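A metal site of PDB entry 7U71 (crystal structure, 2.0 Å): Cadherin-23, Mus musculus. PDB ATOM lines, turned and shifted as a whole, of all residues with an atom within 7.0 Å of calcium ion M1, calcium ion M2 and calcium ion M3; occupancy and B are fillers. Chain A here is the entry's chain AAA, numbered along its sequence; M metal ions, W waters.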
ATOM      1  N   GLU A  18       4.953   3.282 -24.925  1.00  0.00           N
ATOM      2  CA  GLU A  18       5.105   1.918 -25.478  1.00  0.00           C
ATOM      3  C   GLU A  18       4.874   1.963 -27.005  1.00  0.00           C
ATOM      4  O   GLU A  18       4.225   2.916 -27.483  1.00  0.00           O
ATOM      5  CB  GLU A  18       4.187   0.920 -24.779  1.00  0.00           C
ATOM      6  CG  GLU A  18       2.698   1.166 -24.978  1.00  0.00           C
ATOM      7  CD  GLU A  18       1.898   0.016 -24.422  1.00  0.00           C
ATOM      8  OE1 GLU A  18       0.754   0.254 -23.930  1.00  0.00           O
ATOM      9  OE2 GLU A  18       2.438  -1.150 -24.480  1.00  0.00           O
ATOM     10  N   ASN A  19       5.448   0.991 -27.721  1.00  0.00           N
ATOM     11  CA  ASN A  19       5.252   0.776 -29.178  1.00  0.00           C
ATOM     12  C   ASN A  19       5.963   1.903 -29.959  1.00  0.00           C
ATOM     13  O   ASN A  19       5.701   2.066 -31.147  1.00  0.00           O
ATOM     14  CB  ASN A  19       3.776   0.686 -29.545  1.00  0.00           C
ATOM     15  CG  ASN A  19       3.067  -0.396 -28.755  1.00  0.00           C
ATOM     16  OD1 ASN A  19       3.607  -1.482 -28.555  1.00  0.00           O
ATOM     17  ND2 ASN A  19       1.901  -0.087 -28.231  1.00  0.00           N
ATOM     18  N   VAL A  71       8.925  -2.151 -27.380  1.00  0.00           N
ATOM     19  CA  VAL A  71       8.678  -1.735 -25.969  1.00  0.00           C
ATOM     20  C   VAL A  71       7.162  -1.878 -25.694  1.00  0.00           C
ATOM     21  O   VAL A  71       6.351  -1.196 -26.337  1.00  0.00           O
ATOM     22  CB  VAL A  71       9.193  -0.303 -25.720  1.00  0.00           C
ATOM     23  CG1 VAL A  71       8.967   0.132 -24.287  1.00  0.00           C
ATOM     24  CG2 VAL A  71      10.676  -0.181 -26.104  1.00  0.00           C
ATOM     25  N   ASP A  72       6.826  -2.816 -24.825  1.00  0.00           N
ATOM     26  CA  ASP A  72       5.444  -3.244 -24.497  1.00  0.00           C
ATOM     27  C   ASP A  72       5.268  -3.004 -22.992  1.00  0.00           C
ATOM     28  O   ASP A  72       5.817  -3.787 -22.204  1.00  0.00           O
ATOM     29  CB  ASP A  72       5.226  -4.732 -24.771  1.00  0.00           C
ATOM     30  CG  ASP A  72       3.786  -5.210 -24.544  1.00  0.00           C
ATOM     31  OD1 ASP A  72       2.939  -4.429 -24.033  1.00  0.00           O
ATOM     32  OD2 ASP A  72       3.544  -6.380 -24.852  1.00  0.00           O
ATOM     33  N   ARG A  73       4.496  -1.997 -22.609  1.00  0.00           N
ATOM     34  CA  ARG A  73       4.279  -1.698 -21.169  1.00  0.00           C
ATOM     35  C   ARG A  73       3.679  -2.922 -20.481  1.00  0.00           C
ATOM     36  O   ARG A  73       3.926  -3.042 -19.294  1.00  0.00           O
ATOM     37  CB  ARG A  73       3.324  -0.517 -20.970  1.00  0.00           C
ATOM     38  CG  ARG A  73       3.300   0.035 -19.562  1.00  0.00           C
ATOM     39  CD  ARG A  73       2.004   0.755 -19.218  1.00  0.00           C
ATOM     40  NE  ARG A  73       0.940  -0.223 -19.184  1.00  0.00           N
ATOM     41  CZ  ARG A  73       0.631  -1.041 -18.188  1.00  0.00           C
ATOM     42  NH1 ARG A  73       1.192  -0.917 -17.003  1.00  0.00           N
ATOM     43  NH2 ARG A  73      -0.323  -1.933 -18.373  1.00  0.00           N
ATOM     44  N   GLU A  74       2.837  -3.705 -21.170  1.00  0.00           N
ATOM     45  CA  GLU A  74       2.195  -4.872 -20.522  1.00  0.00           C
ATOM     46  C   GLU A  74       3.264  -5.926 -20.222  1.00  0.00           C
ATOM     47  O   GLU A  74       2.907  -6.876 -19.490  1.00  0.00           O
ATOM     48  CB  GLU A  74       1.043  -5.434 -21.372  1.00  0.00           C
ATOM     49  CG  GLU A  74      -0.208  -4.567 -21.308  1.00  0.00           C
ATOM     50  CD  GLU A  74      -0.138  -3.209 -21.986  1.00  0.00           C
ATOM     51  OE1 GLU A  74       0.149  -3.134 -23.208  1.00  0.00           O
ATOM     52  OE2 GLU A  74      -0.398  -2.211 -21.278  1.00  0.00           O
ATOM     53  N   LYS A  75       4.502  -5.802 -20.747  1.00  0.00           N
ATOM     54  CA  LYS A  75       5.612  -6.740 -20.369  1.00  0.00           C
ATOM     55  C   LYS A  75       6.567  -6.104 -19.360  1.00  0.00           C
ATOM     56  O   LYS A  75       7.420  -6.816 -18.867  1.00  0.00           O
ATOM     57  CB  LYS A  75       6.386  -7.197 -21.617  1.00  0.00           C
ATOM     58  CG  LYS A  75       5.651  -8.202 -22.481  1.00  0.00           C
ATOM     59  CD  LYS A  75       6.493  -8.675 -23.659  1.00  0.00           C
ATOM     60  CE  LYS A  75       5.683  -9.058 -24.879  1.00  0.00           C
ATOM     61  NZ  LYS A  75       4.762 -10.183 -24.606  1.00  0.00           N
ATOM     62  N   LEU A 103       5.260   4.526 -20.735  1.00  0.00           N
ATOM     63  CA  LEU A 103       3.827   4.895 -20.568  1.00  0.00           C
ATOM     64  C   LEU A 103       2.929   3.974 -21.411  1.00  0.00           C
ATOM     65  O   LEU A 103       3.383   3.325 -22.356  1.00  0.00           O
ATOM     66  CB  LEU A 103       3.639   6.381 -20.926  1.00  0.00           C
ATOM     67  CG  LEU A 103       4.555   7.352 -20.197  1.00  0.00           C
ATOM     68  CD1 LEU A 103       4.258   8.777 -20.686  1.00  0.00           C
ATOM     69  CD2 LEU A 103       4.325   7.245 -18.698  1.00  0.00           C
ATOM     70  N   ASP A 104       1.655   3.967 -21.064  1.00  0.00           N
ATOM     71  CA  ASP A 104       0.606   3.077 -21.604  1.00  0.00           C
ATOM     72  C   ASP A 104      -0.018   3.659 -22.864  1.00  0.00           C
ATOM     73  O   ASP A 104      -0.415   4.803 -22.842  1.00  0.00           O
ATOM     74  CB  ASP A 104      -0.501   2.893 -20.582  1.00  0.00           C
ATOM     75  CG  ASP A 104      -1.457   1.778 -20.949  1.00  0.00           C
ATOM     76  OD1 ASP A 104      -0.988   0.724 -21.387  1.00  0.00           O
ATOM     77  OD2 ASP A 104      -2.661   1.977 -20.761  1.00  0.00           O
ATOM     78  N   GLU A 105      -0.143   2.865 -23.897  1.00  0.00           N
ATOM     79  CA  GLU A 105      -1.113   3.044 -25.011  1.00  0.00           C
ATOM     80  C   GLU A 105      -2.341   2.162 -24.749  1.00  0.00           C
ATOM     81  O   GLU A 105      -2.198   1.065 -24.169  1.00  0.00           O
ATOM     82  CB  GLU A 105      -0.509   2.612 -26.350  1.00  0.00           C
ATOM     83  CG  GLU A 105       0.607   3.525 -26.820  1.00  0.00           C
ATOM     84  CD  GLU A 105       0.852   3.494 -28.324  1.00  0.00           C
ATOM     85  OE1 GLU A 105       0.748   2.408 -28.933  1.00  0.00           O
ATOM     86  OE2 GLU A 105       1.163   4.588 -28.874  1.00  0.00           O
ATOM     87  N   ASN A 106      -3.504   2.630 -25.133  1.00  0.00           N
ATOM     88  CA  ASN A 106      -4.718   1.789 -25.138  1.00  0.00           C
ATOM     89  C   ASN A 106      -4.597   0.810 -26.298  1.00  0.00           C
ATOM     90  O   ASN A 106      -5.327   0.952 -27.300  1.00  0.00           O
ATOM     91  CB  ASN A 106      -5.993   2.598 -25.220  1.00  0.00           C
ATOM     92  CG  ASN A 106      -7.167   1.717 -24.842  1.00  0.00           C
ATOM     93  OD1 ASN A 106      -6.988   0.649 -24.225  1.00  0.00           O
ATOM     94  ND2 ASN A 106      -8.351   2.124 -25.241  1.00  0.00           N
ATOM     95  N   ASP A 107      -3.711  -0.193 -26.182  1.00  0.00           N
ATOM     96  CA  ASP A 107      -3.445  -1.115 -27.305  1.00  0.00           C
ATOM     97  C   ASP A 107      -4.091  -2.468 -27.049  1.00  0.00           C
ATOM     98  O   ASP A 107      -3.865  -3.365 -27.867  1.00  0.00           O
ATOM     99  CB  ASP A 107      -1.949  -1.191 -27.635  1.00  0.00           C
ATOM    100  CG  ASP A 107      -1.015  -1.649 -26.508  1.00  0.00           C
ATOM    101  OD1 ASP A 107      -1.426  -1.654 -25.298  1.00  0.00           O
ATOM    102  OD2 ASP A 107       0.150  -1.943 -26.849  1.00  0.00           O
ATOM    103  N   ASN A 108      -4.944  -2.617 -26.026  1.00  0.00           N
ATOM    104  CA  ASN A 108      -5.626  -3.907 -25.777  1.00  0.00           C
ATOM    105  C   ASN A 108      -7.129  -3.650 -25.631  1.00  0.00           C
ATOM    106  O   ASN A 108      -7.520  -2.583 -25.124  1.00  0.00           O
ATOM    107  CB  ASN A 108      -5.056  -4.641 -24.562  1.00  0.00           C
ATOM    108  CG  ASN A 108      -3.627  -5.109 -24.792  1.00  0.00           C
ATOM    109  OD1 ASN A 108      -3.431  -6.209 -25.327  1.00  0.00           O
ATOM    110  ND2 ASN A 108      -2.642  -4.266 -24.525  1.00  0.00           N
ATOM    111  N   SER A 109      -7.931  -4.583 -26.166  1.00  0.00           N
ATOM    112  CA  SER A 109      -9.393  -4.601 -26.025  1.00  0.00           C
ATOM    113  C   SER A 109      -9.708  -5.523 -24.858  1.00  0.00           C
ATOM    114  O   SER A 109      -8.888  -6.361 -24.526  1.00  0.00           O
ATOM    115  CB  SER A 109     -10.114  -5.080 -27.293  1.00  0.00           C
ATOM    116  OG  SER A 109      -9.713  -4.269 -28.362  1.00  0.00           O
ATOM    117  N   PRO A 110     -10.880  -5.355 -24.205  1.00  0.00           N
ATOM    118  CA  PRO A 110     -11.327  -6.345 -23.236  1.00  0.00           C
ATOM    119  C   PRO A 110     -11.486  -7.709 -23.907  1.00  0.00           C
ATOM    120  O   PRO A 110     -11.839  -7.779 -25.070  1.00  0.00           O
ATOM    121  CB  PRO A 110     -12.655  -5.781 -22.773  1.00  0.00           C
ATOM    122  CG  PRO A 110     -12.591  -4.268 -23.034  1.00  0.00           C
ATOM    123  CD  PRO A 110     -11.745  -4.158 -24.286  1.00  0.00           C
ATOM    124  N   ASP A 139      -8.841  -6.500 -19.283  1.00  0.00           N
ATOM    125  CA  ASP A 139      -8.155  -5.556 -20.185  1.00  0.00           C
ATOM    126  C   ASP A 139      -6.849  -5.238 -19.467  1.00  0.00           C
ATOM    127  O   ASP A 139      -6.861  -4.798 -18.336  1.00  0.00           O
ATOM    128  CB  ASP A 139      -9.026  -4.315 -20.446  1.00  0.00           C
ATOM    129  CG  ASP A 139      -8.420  -3.400 -21.497  1.00  0.00           C
ATOM    130  OD1 ASP A 139      -7.198  -3.150 -21.419  1.00  0.00           O
ATOM    131  OD2 ASP A 139      -9.195  -2.942 -22.399  1.00  0.00           O
ATOM    132  N   PRO A 140      -5.706  -5.624 -20.019  1.00  0.00           N
ATOM    133  CA  PRO A 140      -4.446  -5.490 -19.286  1.00  0.00           C
ATOM    134  C   PRO A 140      -3.793  -4.106 -19.424  1.00  0.00           C
ATOM    135  O   PRO A 140      -2.707  -3.918 -18.895  1.00  0.00           O
ATOM    136  CB  PRO A 140      -3.613  -6.583 -19.959  1.00  0.00           C
ATOM    137  CG  PRO A 140      -4.066  -6.569 -21.391  1.00  0.00           C
ATOM    138  CD  PRO A 140      -5.552  -6.280 -21.331  1.00  0.00           C
ATOM    139  N   ASP A 141      -4.454  -3.135 -20.065  1.00  0.00           N
ATOM    140  CA  ASP A 141      -3.894  -1.760 -20.103  1.00  0.00           C
ATOM    141  C   ASP A 141      -3.960  -1.128 -18.692  1.00  0.00           C
ATOM    142  O   ASP A 141      -4.599  -1.695 -17.776  1.00  0.00           O
ATOM    143  CB  ASP A 141      -4.557  -0.928 -21.192  1.00  0.00           C
ATOM    144  CG  ASP A 141      -4.344  -1.469 -22.578  1.00  0.00           C
ATOM    145  OD1 ASP A 141      -3.204  -1.876 -22.870  1.00  0.00           O
ATOM    146  OD2 ASP A 141      -5.341  -1.548 -23.357  1.00  0.00           O
ATOM    147  N   ALA A 142      -3.419   0.065 -18.519  1.00  0.00           N
ATOM    148  CA  ALA A 142      -3.296   0.756 -17.209  1.00  0.00           C
ATOM    149  C   ALA A 142      -4.450   1.751 -17.074  1.00  0.00           C
ATOM    150  O   ALA A 142      -4.939   2.268 -18.116  1.00  0.00           O
ATOM    151  CB  ALA A 142      -1.922   1.431 -17.090  1.00  0.00           C
ATOM    152  N   SER A 144      -7.676   3.918 -16.804  1.00  0.00           N
ATOM    153  CA  SER A 144      -8.929   3.964 -17.608  1.00  0.00           C
ATOM    154  C   SER A 144      -8.873   2.974 -18.792  1.00  0.00           C
ATOM    155  O   SER A 144      -9.893   2.366 -19.147  1.00  0.00           O
ATOM    156  CB  SER A 144      -9.121   5.361 -18.169  1.00  0.00           C
ATOM    157  OG  SER A 144      -9.496   6.274 -17.163  1.00  0.00           O
ATOM    158  N   ASN A 145      -7.731   2.936 -19.478  1.00  0.00           N
ATOM    159  CA  ASN A 145      -7.473   2.060 -20.662  1.00  0.00           C
ATOM    160  C   ASN A 145      -7.723   0.603 -20.306  1.00  0.00           C
ATOM    161  O   ASN A 145      -7.968  -0.178 -21.233  1.00  0.00           O
ATOM    162  CB  ASN A 145      -6.054   2.185 -21.216  1.00  0.00           C
ATOM    163  CG  ASN A 145      -5.753   3.574 -21.734  1.00  0.00           C
ATOM    164  OD1 ASN A 145      -6.669   4.324 -22.106  1.00  0.00           O
ATOM    165  ND2 ASN A 145      -4.467   3.921 -21.780  1.00  0.00           N
ATOM    166  N   GLY A 146      -7.650   0.259 -19.017  1.00  0.00           N
ATOM    167  CA  GLY A 146      -7.845  -1.116 -18.536  1.00  0.00           C
ATOM    168  C   GLY A 146      -9.104  -1.334 -17.722  1.00  0.00           C
ATOM    169  O   GLY A 146      -9.331  -2.484 -17.310  1.00  0.00           O
ATOM    170  N   GLN A 147      -9.871  -0.299 -17.423  1.00  0.00           N
ATOM    171  CA  GLN A 147     -11.138  -0.485 -16.667  1.00  0.00           C
ATOM    172  C   GLN A 147     -12.243  -0.977 -17.603  1.00  0.00           C
ATOM    173  O   GLN A 147     -12.367  -0.377 -18.655  1.00  0.00           O
ATOM    174  CB  GLN A 147     -11.612   0.867 -16.137  1.00  0.00           C
ATOM    175  CG  GLN A 147     -10.835   1.333 -14.935  1.00  0.00           C
ATOM    176  CD  GLN A 147     -11.315   2.713 -14.559  1.00  0.00           C
ATOM    177  OE1 GLN A 147     -11.667   3.537 -15.392  1.00  0.00           O
ATOM    178  NE2 GLN A 147     -11.411   2.948 -13.262  1.00  0.00           N
ATOM    179  N   ASP A 195     -13.678  -0.823 -22.611  1.00  0.00           N
ATOM    180  CA  ASP A 195     -12.733  -0.159 -21.677  1.00  0.00           C
ATOM    181  C   ASP A 195     -13.142   1.313 -21.533  1.00  0.00           C
ATOM    182  O   ASP A 195     -14.169   1.730 -22.095  1.00  0.00           O
ATOM    183  CB  ASP A 195     -11.263  -0.399 -22.036  1.00  0.00           C
ATOM    184  CG  ASP A 195     -10.746   0.248 -23.311  1.00  0.00           C
ATOM    185  OD1 ASP A 195     -11.327   1.311 -23.744  1.00  0.00           O
ATOM    186  OD2 ASP A 195      -9.760  -0.326 -23.873  1.00  0.00           O
ATOM    187  N   ARG A 196     -12.402   2.085 -20.748  1.00  0.00           N
ATOM    188  CA  ARG A 196     -12.688   3.526 -20.576  1.00  0.00           C
ATOM    189  C   ARG A 196     -11.566   4.313 -21.243  1.00  0.00           C
ATOM    190  O   ARG A 196     -11.284   5.433 -20.823  1.00  0.00           O
ATOM    191  CB  ARG A 196     -12.882   3.820 -19.090  1.00  0.00           C
ATOM    192  CG  ARG A 196     -14.145   3.188 -18.509  1.00  0.00           C
ATOM    193  CD  ARG A 196     -14.683   3.941 -17.297  1.00  0.00           C
ATOM    194  NE  ARG A 196     -15.688   3.204 -16.516  1.00  0.00           N
ATOM    195  CZ  ARG A 196     -17.009   3.284 -16.638  1.00  0.00           C
ATOM    196  NH1 ARG A 196     -17.562   4.068 -17.532  1.00  0.00           N
ATOM    197  NH2 ARG A 196     -17.791   2.584 -15.816  1.00  0.00           N
ATOM    198  N   GLY A 197     -10.977   3.741 -22.271  1.00  0.00           N
ATOM    199  CA  GLY A 197     -10.062   4.511 -23.104  1.00  0.00           C
ATOM    200  C   GLY A 197     -10.810   5.653 -23.758  1.00  0.00           C
ATOM    201  O   GLY A 197     -12.048   5.598 -23.867  1.00  0.00           O
ATOM    202  N   ARG A 201     -12.139   0.993 -26.459  1.00  0.00           N
ATOM    203  CA  ARG A 201     -12.082  -0.269 -27.226  1.00  0.00           C
ATOM    204  C   ARG A 201     -13.139  -1.226 -26.685  1.00  0.00           C
ATOM    205  O   ARG A 201     -13.323  -1.309 -25.466  1.00  0.00           O
ATOM    206  CB  ARG A 201     -10.651  -0.766 -27.135  1.00  0.00           C
ATOM    207  CG  ARG A 201      -9.681   0.041 -27.996  1.00  0.00           C
ATOM    208  CD  ARG A 201      -8.274  -0.448 -27.789  1.00  0.00           C
ATOM    209  NE  ARG A 201      -8.083  -1.699 -28.466  1.00  0.00           N
ATOM    210  CZ  ARG A 201      -7.106  -1.985 -29.315  1.00  0.00           C
ATOM    211  NH1 ARG A 201      -6.148  -1.124 -29.613  1.00  0.00           N
ATOM    212  NH2 ARG A 201      -7.108  -3.164 -29.887  1.00  0.00           N
HETATM  213 CA    CA M   1      -7.743  -1.373 -23.159  1.00  0.00          CA
HETATM  214 CA    CA M   2      -1.083  -0.793 -23.122  1.00  0.00          CA
HETATM  215 CA    CA M   3       1.338  -3.095 -25.149  1.00  0.00          CA
HETATM  216  O   HOH W   1       2.850  -3.477 -26.916  1.00  0.00           O
HETATM  217  O   HOH W   2       0.065  -5.235 -25.562  1.00  0.00           O
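Six residues have an atom within 4 Å of calcium ion M2: Glu 18, Glu 74, Asp 104, Glu 105, Asp 107 and Asp 141.
Calcium ion M1 is bound by OD2 of Asp 139, O of Asn 145, O of Asn 108, OD2 of Asp 195, OD1 of Asn 106, OD2 of Asp 141 and OD1 of Asp 139.
Calcium ion M1 has seven donor atoms within binding distance.
Within 4 Å of calcium ion M3: Glu 18, Asp 72, Glu 74 and Asp 107.
The nearest printed residue that does not touch calcium ion M3 is Asn 108 (4.2 Å).
Calcium ion M2 is bound by OE1 of Glu 18 (2.3 Å), OD1 of Asp 104 (2.3 Å), OD1 of Asp 107 (2.4 Å), OD1 of Asp 141 (2.4 Å), O of Glu 105 (2.4 Å), OE2 of Glu 74 (2.4 Å) and OE1 of Glu 74 (2.6 Å).
The side-chain carboxylate of Asp 104 sits close to the guanidinium group of Arg 73, at 3.1 Å.
N of Ala 142 lies within hydrogen-bond range of OD2 of Asp 104 (3.0 Å).
ND2 of Asn 108 lies close to OD1 of Asp 107 (3.0 Å).
N of Glu 18 sits at hydrogen-bond distance from O of Leu 103 (3.0 Å).
The side-chain carboxylate (OE1) of Glu 105 sits at hydrogen-bond distance from the side-chain amide nitrogen (ND2) of Asn 19, 2.8 Å away.
The side-chain carboxylate (OD2) of Asp 107 lies close to the side-chain amide nitrogen (ND2) of Asn 19, at 2.9 Å.
The side-chain carboxylate (OD2) of Asp 104 sits at hydrogen-bond distance from the side-chain amide nitrogen (ND2) of Asn 145 (2.8 Å).
The side-chain carboxylate (OE2) of Glu 18 lies close to the backbone NH (N) of Arg 73.
Of the 27 residues printed, 6 come within 4 Å of calcium ion M1.
Calcium ion M3 is bound by the side-chain carboxylate of Glu 74, the side-chain carboxylate of Glu 18, water W1, the side-chain carboxylate of Asp 72, the side-chain carboxylate of Asp 107 and water W2.
Calcium ion M3 has six donor atoms within binding distance.
Slightly farther from calcium ion M3 lies OD1 of Asp 107 (3.1 Å).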
